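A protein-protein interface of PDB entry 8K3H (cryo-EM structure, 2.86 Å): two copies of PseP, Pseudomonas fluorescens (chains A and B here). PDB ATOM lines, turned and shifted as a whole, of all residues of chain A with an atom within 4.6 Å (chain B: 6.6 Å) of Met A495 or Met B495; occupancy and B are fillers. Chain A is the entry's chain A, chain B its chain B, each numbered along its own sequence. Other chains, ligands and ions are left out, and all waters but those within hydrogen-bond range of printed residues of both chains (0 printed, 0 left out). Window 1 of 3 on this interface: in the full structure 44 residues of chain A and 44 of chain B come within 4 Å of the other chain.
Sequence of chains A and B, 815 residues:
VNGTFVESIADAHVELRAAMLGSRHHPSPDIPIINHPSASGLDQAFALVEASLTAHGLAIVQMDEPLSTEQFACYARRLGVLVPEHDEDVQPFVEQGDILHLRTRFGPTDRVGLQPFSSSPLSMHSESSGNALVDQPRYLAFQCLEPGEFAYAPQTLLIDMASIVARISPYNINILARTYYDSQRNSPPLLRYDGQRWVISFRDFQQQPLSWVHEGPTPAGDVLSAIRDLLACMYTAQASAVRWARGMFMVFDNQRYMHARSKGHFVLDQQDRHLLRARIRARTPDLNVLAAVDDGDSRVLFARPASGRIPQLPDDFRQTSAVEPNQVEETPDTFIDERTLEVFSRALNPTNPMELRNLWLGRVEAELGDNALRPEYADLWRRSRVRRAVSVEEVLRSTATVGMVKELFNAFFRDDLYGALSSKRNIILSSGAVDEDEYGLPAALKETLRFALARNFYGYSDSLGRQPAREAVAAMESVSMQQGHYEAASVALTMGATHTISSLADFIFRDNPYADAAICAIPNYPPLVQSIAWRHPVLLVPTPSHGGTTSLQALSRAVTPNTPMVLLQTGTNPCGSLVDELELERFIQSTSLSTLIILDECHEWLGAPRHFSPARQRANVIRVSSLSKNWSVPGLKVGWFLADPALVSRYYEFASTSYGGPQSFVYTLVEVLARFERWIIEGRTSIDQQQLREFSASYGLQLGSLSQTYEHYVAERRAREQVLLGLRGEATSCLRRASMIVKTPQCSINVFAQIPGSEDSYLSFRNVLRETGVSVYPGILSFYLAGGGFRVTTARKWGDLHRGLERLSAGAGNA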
ATOM      1  N   THR A 494     -23.529 -22.783  14.216  1.00  0.00           N
ATOM      2  CA  THR A 494     -23.015 -22.205  15.449  1.00  0.00           C
ATOM      3  C   THR A 494     -23.798 -22.756  16.633  1.00  0.00           C
ATOM      4  O   THR A 494     -24.794 -23.467  16.473  1.00  0.00           O
ATOM      5  CB  THR A 494     -23.088 -20.672  15.432  1.00  0.00           C
ATOM      6  OG1 THR A 494     -24.412 -20.258  15.075  1.00  0.00           O
ATOM      7  CG2 THR A 494     -22.090 -20.094  14.439  1.00  0.00           C
ATOM      8  N   MET A 495     -23.329 -22.425  17.834  1.00  0.00           N
ATOM      9  CA  MET A 495     -23.923 -22.928  19.073  1.00  0.00           C
ATOM     10  C   MET A 495     -24.878 -21.892  19.667  1.00  0.00           C
ATOM     11  O   MET A 495     -24.658 -21.337  20.744  1.00  0.00           O
ATOM     12  CB  MET A 495     -22.828 -23.316  20.062  1.00  0.00           C
ATOM     13  CG  MET A 495     -21.611 -23.959  19.421  1.00  0.00           C
ATOM     14  SD  MET A 495     -20.460 -24.634  20.633  1.00  0.00           S
ATOM     15  CE  MET A 495     -19.462 -23.191  20.988  1.00  0.00           C
ATOM     16  N   GLY A 496     -25.963 -21.642  18.941  1.00  0.00           N
ATOM     17  CA  GLY A 496     -27.017 -20.772  19.417  1.00  0.00           C
ATOM     18  C   GLY A 496     -26.835 -19.322  19.001  1.00  0.00           C
ATOM     19  O   GLY A 496     -25.762 -18.880  18.585  1.00  0.00           O
ATOM     20  N   ALA A 497     -27.927 -18.565  19.130  1.00  0.00           N
ATOM     21  CA  ALA A 497     -27.943 -17.179  18.675  1.00  0.00           C
ATOM     22  C   ALA A 497     -27.128 -16.266  19.583  1.00  0.00           C
ATOM     23  O   ALA A 497     -26.467 -15.340  19.098  1.00  0.00           O
ATOM     24  CB  ALA A 497     -29.382 -16.676  18.573  1.00  0.00           C
ATOM     25  N   HIS A 499     -24.447 -17.076  21.342  1.00  0.00           N
ATOM     26  CA  HIS A 499     -23.045 -17.311  21.019  1.00  0.00           C
ATOM     27  C   HIS A 499     -22.705 -16.831  19.614  1.00  0.00           C
ATOM     28  O   HIS A 499     -21.584 -16.370  19.375  1.00  0.00           O
ATOM     29  CB  HIS A 499     -22.718 -18.796  21.175  1.00  0.00           C
ATOM     30  CG  HIS A 499     -21.340 -19.164  20.721  1.00  0.00           C
ATOM     31  ND1 HIS A 499     -20.217 -18.917  21.480  1.00  0.00           N
ATOM     32  CD2 HIS A 499     -20.904 -19.761  19.586  1.00  0.00           C
ATOM     33  CE1 HIS A 499     -19.148 -19.345  20.832  1.00  0.00           C
ATOM     34  NE2 HIS A 499     -19.538 -19.861  19.680  1.00  0.00           N
ATOM     35  N   LYS A 637     -28.240 -25.754  22.172  1.00  0.00           N
ATOM     36  CA  LYS A 637     -27.278 -24.804  21.615  1.00  0.00           C
ATOM     37  C   LYS A 637     -27.014 -25.093  20.137  1.00  0.00           C
ATOM     38  O   LYS A 637     -25.896 -25.399  19.720  1.00  0.00           O
ATOM     39  CB  LYS A 637     -25.976 -24.812  22.421  1.00  0.00           C
ATOM     40  CG  LYS A 637     -26.057 -24.076  23.744  1.00  0.00           C
ATOM     41  CD  LYS A 637     -26.155 -22.578  23.532  1.00  0.00           C
ATOM     42  CE  LYS A 637     -26.061 -21.833  24.848  1.00  0.00           C
ATOM     43  NZ  LYS A 637     -24.676 -21.851  25.388  1.00  0.00           N
ATOM     44  N   VAL A 638     -28.077 -24.993  19.344  1.00  0.00           N
ATOM     45  CA  VAL A 638     -28.035 -25.292  17.918  1.00  0.00           C
ATOM     46  C   VAL A 638     -28.498 -24.066  17.143  1.00  0.00           C
ATOM     47  O   VAL A 638     -29.534 -23.474  17.461  1.00  0.00           O
ATOM     48  CB  VAL A 638     -28.905 -26.517  17.568  1.00  0.00           C
ATOM     49  CG1 VAL A 638     -28.856 -26.795  16.075  1.00  0.00           C
ATOM     50  CG2 VAL A 638     -28.451 -27.732  18.358  1.00  0.00           C
ATOM     51  N   TYR A 659     -13.757 -21.869  19.366  1.00  0.00           N
ATOM     52  CA  TYR A 659     -14.364 -23.051  19.961  1.00  0.00           C
ATOM     53  C   TYR A 659     -14.080 -24.345  19.215  1.00  0.00           C
ATOM     54  O   TYR A 659     -14.529 -25.402  19.670  1.00  0.00           O
ATOM     55  CB  TYR A 659     -15.887 -22.871  20.089  1.00  0.00           C
ATOM     56  CG  TYR A 659     -16.577 -22.363  18.841  1.00  0.00           C
ATOM     57  CD1 TYR A 659     -16.653 -21.004  18.570  1.00  0.00           C
ATOM     58  CD2 TYR A 659     -17.167 -23.243  17.944  1.00  0.00           C
ATOM     59  CE1 TYR A 659     -17.285 -20.537  17.436  1.00  0.00           C
ATOM     60  CE2 TYR A 659     -17.802 -22.784  16.808  1.00  0.00           C
ATOM     61  CZ  TYR A 659     -17.858 -21.431  16.559  1.00  0.00           C
ATOM     62  OH  TYR A 659     -18.490 -20.969  15.429  1.00  0.00           O
ATOM     63  N   GLY A 661     -15.314 -25.698  16.608  1.00  0.00           N
ATOM     64  CA  GLY A 661     -16.369 -26.071  15.697  1.00  0.00           C
ATOM     65  C   GLY A 661     -17.679 -26.306  16.418  1.00  0.00           C
ATOM     66  O   GLY A 661     -17.739 -26.335  17.650  1.00  0.00           O
ATOM     67  N   PRO A 662     -18.756 -26.480  15.662  1.00  0.00           N
ATOM     68  CA  PRO A 662     -20.072 -26.681  16.271  1.00  0.00           C
ATOM     69  C   PRO A 662     -20.219 -28.088  16.838  1.00  0.00           C
ATOM     70  O   PRO A 662     -19.284 -28.888  16.864  1.00  0.00           O
ATOM     71  CB  PRO A 662     -21.038 -26.457  15.106  1.00  0.00           C
ATOM     72  CG  PRO A 662     -20.242 -26.825  13.901  1.00  0.00           C
ATOM     73  CD  PRO A 662     -18.833 -26.400  14.194  1.00  0.00           C
ATOM     74  N   LEU B 493     -19.244 -25.010  34.644  1.00  0.00           N
ATOM     75  CA  LEU B 493     -19.352 -25.860  33.467  1.00  0.00           C
ATOM     76  C   LEU B 493     -19.219 -25.033  32.194  1.00  0.00           C
ATOM     77  O   LEU B 493     -19.780 -23.941  32.081  1.00  0.00           O
ATOM     78  CB  LEU B 493     -20.686 -26.606  33.473  1.00  0.00           C
ATOM     79  CG  LEU B 493     -21.023 -27.386  34.745  1.00  0.00           C
ATOM     80  CD1 LEU B 493     -22.359 -28.094  34.603  1.00  0.00           C
ATOM     81  CD2 LEU B 493     -19.922 -28.380  35.077  1.00  0.00           C
ATOM     82  N   THR B 494     -18.466 -25.562  31.229  1.00  0.00           N
ATOM     83  CA  THR B 494     -18.211 -24.871  29.974  1.00  0.00           C
ATOM     84  C   THR B 494     -18.357 -25.850  28.817  1.00  0.00           C
ATOM     85  O   THR B 494     -18.522 -27.057  29.010  1.00  0.00           O
ATOM     86  CB  THR B 494     -16.818 -24.227  29.952  1.00  0.00           C
ATOM     87  OG1 THR B 494     -15.833 -25.200  30.320  1.00  0.00           O
ATOM     88  CG2 THR B 494     -16.750 -23.050  30.916  1.00  0.00           C
ATOM     89  N   MET B 495     -18.298 -25.311  27.600  1.00  0.00           N
ATOM     90  CA  MET B 495     -18.489 -26.101  26.385  1.00  0.00           C
ATOM     91  C   MET B 495     -17.139 -26.482  25.777  1.00  0.00           C
ATOM     92  O   MET B 495     -16.766 -26.055  24.685  1.00  0.00           O
ATOM     93  CB  MET B 495     -19.355 -25.336  25.389  1.00  0.00           C
ATOM     94  CG  MET B 495     -20.476 -24.534  26.029  1.00  0.00           C
ATOM     95  SD  MET B 495     -21.624 -23.856  24.817  1.00  0.00           S
ATOM     96  CE  MET B 495     -20.806 -22.318  24.405  1.00  0.00           C
ATOM     97  N   GLY B 496     -16.403 -27.311  26.511  1.00  0.00           N
ATOM     98  CA  GLY B 496     -15.150 -27.851  26.028  1.00  0.00           C
ATOM     99  C   GLY B 496     -13.945 -27.009  26.410  1.00  0.00           C
ATOM    100  O   GLY B 496     -14.047 -25.849  26.813  1.00  0.00           O
ATOM    101  N   ALA B 497     -12.768 -27.624  26.267  1.00  0.00           N
ATOM    102  CA  ALA B 497     -11.528 -26.986  26.694  1.00  0.00           C
ATOM    103  C   ALA B 497     -11.102 -25.866  25.752  1.00  0.00           C
ATOM    104  O   ALA B 497     -10.578 -24.843  26.203  1.00  0.00           O
ATOM    105  CB  ALA B 497     -10.416 -28.028  26.814  1.00  0.00           C
ATOM    106  N   THR B 498     -11.304 -26.044  24.443  1.00  0.00           N
ATOM    107  CA  THR B 498     -10.955 -24.989  23.496  1.00  0.00           C
ATOM    108  C   THR B 498     -11.787 -23.738  23.739  1.00  0.00           C
ATOM    109  O   THR B 498     -11.264 -22.618  23.713  1.00  0.00           O
ATOM    110  CB  THR B 498     -11.137 -25.480  22.061  1.00  0.00           C
ATOM    111  OG1 THR B 498     -10.486 -26.746  21.899  1.00  0.00           O
ATOM    112  CG2 THR B 498     -10.546 -24.484  21.075  1.00  0.00           C
ATOM    113  N   HIS B 499     -13.088 -23.910  23.976  1.00  0.00           N
ATOM    114  CA  HIS B 499     -13.942 -22.769  24.282  1.00  0.00           C
ATOM    115  C   HIS B 499     -13.652 -22.209  25.670  1.00  0.00           C
ATOM    116  O   HIS B 499     -13.760 -20.996  25.880  1.00  0.00           O
ATOM    117  CB  HIS B 499     -15.412 -23.171  24.160  1.00  0.00           C
ATOM    118  CG  HIS B 499     -16.369 -22.110  24.603  1.00  0.00           C
ATOM    119  ND1 HIS B 499     -16.684 -21.019  23.821  1.00  0.00           N
ATOM    120  CD2 HIS B 499     -17.082 -21.972  25.746  1.00  0.00           C
ATOM    121  CE1 HIS B 499     -17.548 -20.254  24.464  1.00  0.00           C
ATOM    122  NE2 HIS B 499     -17.806 -20.810  25.633  1.00  0.00           N
ATOM    123  N   THR B 500     -13.288 -23.071  26.623  1.00  0.00           N
ATOM    124  CA  THR B 500     -13.002 -22.612  27.980  1.00  0.00           C
ATOM    125  C   THR B 500     -11.800 -21.677  28.004  1.00  0.00           C
ATOM    126  O   THR B 500     -11.862 -20.581  28.574  1.00  0.00           O
ATOM    127  CB  THR B 500     -12.759 -23.809  28.899  1.00  0.00           C
ATOM    128  OG1 THR B 500     -13.871 -24.707  28.826  1.00  0.00           O
ATOM    129  CG2 THR B 500     -12.577 -23.350  30.337  1.00  0.00           C
ATOM    130  N   SER B 626     -11.615 -31.496  30.205  1.00  0.00           N
ATOM    131  CA  SER B 626     -12.629 -31.713  29.184  1.00  0.00           C
ATOM    132  C   SER B 626     -12.889 -33.206  29.052  1.00  0.00           C
ATOM    133  O   SER B 626     -12.089 -34.037  29.491  1.00  0.00           O
ATOM    134  CB  SER B 626     -12.209 -31.119  27.837  1.00  0.00           C
ATOM    135  OG  SER B 626     -13.321 -30.982  26.972  1.00  0.00           O
ATOM    136  N1  LLP B 629      -6.103 -29.300  24.785  1.00  0.00           N
ATOM    137  C2  LLP B 629      -5.353 -30.177  24.122  1.00  0.00           C
ATOM    138  C2' LLP B 629      -3.878 -29.954  24.047  1.00  0.00           C
ATOM    139  C3  LLP B 629      -5.935 -31.291  23.504  1.00  0.00           C
ATOM    140  O3  LLP B 629      -5.120 -32.147  22.843  1.00  0.00           O
ATOM    141  C4  LLP B 629      -7.327 -31.475  23.581  1.00  0.00           C
ATOM    142  C4' LLP B 629      -7.984 -32.625  22.965  1.00  0.00           C
ATOM    143  C5  LLP B 629      -8.089 -30.540  24.296  1.00  0.00           C
ATOM    144  C6  LLP B 629      -7.438 -29.481  24.865  1.00  0.00           C
ATOM    145  C5' LLP B 629      -9.581 -30.672  24.425  1.00  0.00           C
ATOM    146  OP4 LLP B 629     -10.258 -29.706  23.561  1.00  0.00           O
ATOM    147  P   LLP B 629     -11.859 -29.722  23.363  1.00  0.00           P
ATOM    148  OP1 LLP B 629     -12.159 -30.944  22.520  1.00  0.00           O
ATOM    149  OP2 LLP B 629     -12.207 -28.426  22.663  1.00  0.00           O
ATOM    150  OP3 LLP B 629     -12.446 -29.814  24.758  1.00  0.00           O
ATOM    151  N   LLP B 629     -11.157 -36.207  25.344  1.00  0.00           N
ATOM    152  CA  LLP B 629     -10.077 -37.221  25.210  1.00  0.00           C
ATOM    153  CB  LLP B 629      -8.707 -36.574  25.438  1.00  0.00           C
ATOM    154  CG  LLP B 629      -7.988 -36.085  24.186  1.00  0.00           C
ATOM    155  CD  LLP B 629      -8.891 -35.368  23.191  1.00  0.00           C
ATOM    156  CE  LLP B 629      -8.131 -34.765  22.027  1.00  0.00           C
ATOM    157  NZ  LLP B 629      -7.354 -33.607  22.463  1.00  0.00           N
ATOM    158  C   LLP B 629     -10.323 -38.373  26.190  1.00  0.00           C
ATOM    159  O   LLP B 629     -10.404 -39.527  25.726  1.00  0.00           O
ATOM    160  N   LEU B 636     -19.596 -33.534  21.860  1.00  0.00           N
ATOM    161  CA  LEU B 636     -20.573 -33.136  22.860  1.00  0.00           C
ATOM    162  C   LEU B 636     -20.283 -31.768  23.460  1.00  0.00           C
ATOM    163  O   LEU B 636     -21.209 -31.124  23.963  1.00  0.00           O
ATOM    164  CB  LEU B 636     -20.638 -34.178  23.982  1.00  0.00           C
ATOM    165  CG  LEU B 636     -21.679 -35.289  23.823  1.00  0.00           C
ATOM    166  CD1 LEU B 636     -21.779 -36.113  25.095  1.00  0.00           C
ATOM    167  CD2 LEU B 636     -23.033 -34.711  23.451  1.00  0.00           C
ATOM    168  N   LYS B 637     -19.031 -31.315  23.415  1.00  0.00           N
ATOM    169  CA  LYS B 637     -18.629 -30.006  23.929  1.00  0.00           C
ATOM    170  C   LYS B 637     -18.982 -29.866  25.411  1.00  0.00           C
ATOM    171  O   LYS B 637     -19.772 -29.012  25.817  1.00  0.00           O
ATOM    172  CB  LYS B 637     -19.257 -28.879  23.104  1.00  0.00           C
ATOM    173  CG  LYS B 637     -18.597 -28.648  21.758  1.00  0.00           C
ATOM    174  CD  LYS B 637     -17.217 -28.041  21.920  1.00  0.00           C
ATOM    175  CE  LYS B 637     -16.637 -27.641  20.578  1.00  0.00           C
ATOM    176  NZ  LYS B 637     -17.304 -26.431  20.032  1.00  0.00           N
ATOM    177  N   VAL B 638     -18.377 -30.732  26.220  1.00  0.00           N
ATOM    178  CA  VAL B 638     -18.642 -30.799  27.651  1.00  0.00           C
ATOM    179  C   VAL B 638     -17.332 -30.623  28.405  1.00  0.00           C
ATOM    180  O   VAL B 638     -16.329 -31.272  28.088  1.00  0.00           O
ATOM    181  CB  VAL B 638     -19.318 -32.130  28.041  1.00  0.00           C
ATOM    182  CG1 VAL B 638     -19.568 -32.181  29.540  1.00  0.00           C
ATOM    183  CG2 VAL B 638     -20.615 -32.313  27.273  1.00  0.00           C
ATOM    184  N   GLY B 639     -17.344 -29.746  29.400  1.00  0.00           N
ATOM    185  CA  GLY B 639     -16.161 -29.527  30.207  1.00  0.00           C
ATOM    186  C   GLY B 639     -16.467 -28.611  31.369  1.00  0.00           C
ATOM    187  O   GLY B 639     -17.616 -28.223  31.595  1.00  0.00           O
ATOM    188  N   TRP B 640     -15.416 -28.271  32.108  1.00  0.00           N
ATOM    189  CA  TRP B 640     -15.522 -27.374  33.253  1.00  0.00           C
ATOM    190  C   TRP B 640     -14.120 -26.912  33.621  1.00  0.00           C
ATOM    191  O   TRP B 640     -13.124 -27.400  33.082  1.00  0.00           O
ATOM    192  CB  TRP B 640     -16.207 -28.051  34.444  1.00  0.00           C
ATOM    193  CG  TRP B 640     -15.517 -29.299  34.911  1.00  0.00           C
ATOM    194  CD1 TRP B 640     -14.398 -29.376  35.688  1.00  0.00           C
ATOM    195  CD2 TRP B 640     -15.903 -30.649  34.631  1.00  0.00           C
ATOM    196  NE1 TRP B 640     -14.063 -30.688  35.907  1.00  0.00           N
ATOM    197  CE2 TRP B 640     -14.971 -31.491  35.268  1.00  0.00           C
ATOM    198  CE3 TRP B 640     -16.945 -31.228  33.900  1.00  0.00           C
ATOM    199  CZ2 TRP B 640     -15.050 -32.879  35.199  1.00  0.00           C
ATOM    200  CZ3 TRP B 640     -17.022 -32.607  33.833  1.00  0.00           C
ATOM    201  CH2 TRP B 640     -16.081 -33.416  34.479  1.00  0.00           C
ATOM    202  N   TYR B 659     -22.260 -16.611  25.909  1.00  0.00           N
ATOM    203  CA  TYR B 659     -23.034 -17.707  25.348  1.00  0.00           C
ATOM    204  C   TYR B 659     -24.303 -18.040  26.118  1.00  0.00           C
ATOM    205  O   TYR B 659     -25.048 -18.922  25.680  1.00  0.00           O
ATOM    206  CB  TYR B 659     -22.172 -18.976  25.234  1.00  0.00           C
ATOM    207  CG  TYR B 659     -21.382 -19.322  26.479  1.00  0.00           C
ATOM    208  CD1 TYR B 659     -20.139 -18.750  26.717  1.00  0.00           C
ATOM    209  CD2 TYR B 659     -21.872 -20.232  27.405  1.00  0.00           C
ATOM    210  CE1 TYR B 659     -19.414 -19.065  27.849  1.00  0.00           C
ATOM    211  CE2 TYR B 659     -21.153 -20.553  28.538  1.00  0.00           C
ATOM    212  CZ  TYR B 659     -19.926 -19.968  28.755  1.00  0.00           C
ATOM    213  OH  TYR B 659     -19.206 -20.286  29.883  1.00  0.00           O
ATOM    214  N   GLY B 661     -24.887 -19.731  28.765  1.00  0.00           N
ATOM    215  CA  GLY B 661     -24.717 -20.828  29.687  1.00  0.00           C
ATOM    216  C   GLY B 661     -24.331 -22.112  28.987  1.00  0.00           C
ATOM    217  O   GLY B 661     -24.352 -22.207  27.756  1.00  0.00           O
ATOM    218  N   PRO B 662     -23.964 -23.128  29.760  1.00  0.00           N
ATOM    219  CA  PRO B 662     -23.543 -24.402  29.171  1.00  0.00           C
ATOM    220  C   PRO B 662     -24.732 -25.214  28.673  1.00  0.00           C
ATOM    221  O   PRO B 662     -25.886 -24.785  28.709  1.00  0.00           O
ATOM    222  CB  PRO B 662     -22.841 -25.109  30.332  1.00  0.00           C
ATOM    223  CG  PRO B 662     -23.502 -24.552  31.546  1.00  0.00           C
ATOM    224  CD  PRO B 662     -23.813 -23.120  31.223  1.00  0.00           C
ATOM    225  N   GLN B 663     -24.416 -26.417  28.202  1.00  0.00           N
ATOM    226  CA  GLN B 663     -25.416 -27.343  27.684  1.00  0.00           C
ATOM    227  C   GLN B 663     -26.228 -27.901  28.846  1.00  0.00           C
ATOM    228  O   GLN B 663     -25.684 -28.595  29.711  1.00  0.00           O
ATOM    229  CB  GLN B 663     -24.729 -28.475  26.927  1.00  0.00           C
ATOM    230  CG  GLN B 663     -24.015 -28.059  25.655  1.00  0.00           C
ATOM    231  CD  GLN B 663     -23.343 -29.236  24.976  1.00  0.00           C
ATOM    232  OE1 GLN B 663     -23.359 -30.354  25.493  1.00  0.00           O
ATOM    233  NE2 GLN B 663     -22.716 -28.986  23.832  1.00  0.00           N
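The side-chain hydroxyl of Thr B498 is in hydrogen-bond range of OP2 of LLP B629.
Met A495 touches its own counterpart, Met B495. Met A495 touches Lys B637, and with the chains exchanged Lys A637 touches Met B495. Lys A637 touches Tyr B659, and with the chains exchanged Tyr A659 touches Lys B637. Lys A637 touches Gly B661, and with the chains exchanged Gly A661 touches Lys B637. Of the 8 pairs that touch across the chains among the printed residues, 7 have their exchanged pair printed and touching as well.
Of chain B, only Met B495 and Lys B637 come within 4 Å of Met A495. Ala A497 touches none of the printed residues of chain B. Of the printed residues of chain B, Gly A661 touches Lys B637. Of the printed residues of chain A, Met B495 touches Met A495 (3.8 Å) and Lys A637 (3.7 Å). Printed residues of chain A within 4 Å of Tyr B659: Lys A637. The nearest printed residue of chain B that does not touch Lys A637 is Pro B662 (4.6 Å).
Hydrophobic or aromatic side chains of chain A within 4 Å of the printed part of chain B: Met A495 and Tyr A659. Among the printed residues, 8 pairs touch across the chains. Among the printed residues, no Asp or Glu carboxylate lies within 4 Å of a Lys or Arg side-chain nitrogen of the other chain.
NZ of Lys A637 is in hydrogen-bond range of O of Gly B661, at 2.4 Å. O of Gly A661 sits at hydrogen-bond distance from NZ of Lys B637 (2.4 Å). The side-chain amino group (NZ) of Lys B637 is in hydrogen-bond range of the side-chain sulfur (SD) of Met A495 (3.7 Å). O of Tyr A659 sits at hydrogen-bond distance from NZ of Lys B637 (3.0 Å). O of Tyr B659 sits at hydrogen-bond distance from NZ of Lys A637. NZ of Lys A637 is in hydrogen-bond range of SD of Met B495.
Met A495 touches Met B495. Tyr A659 touches Thr B498 (C to CG2, 3.996 Å).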
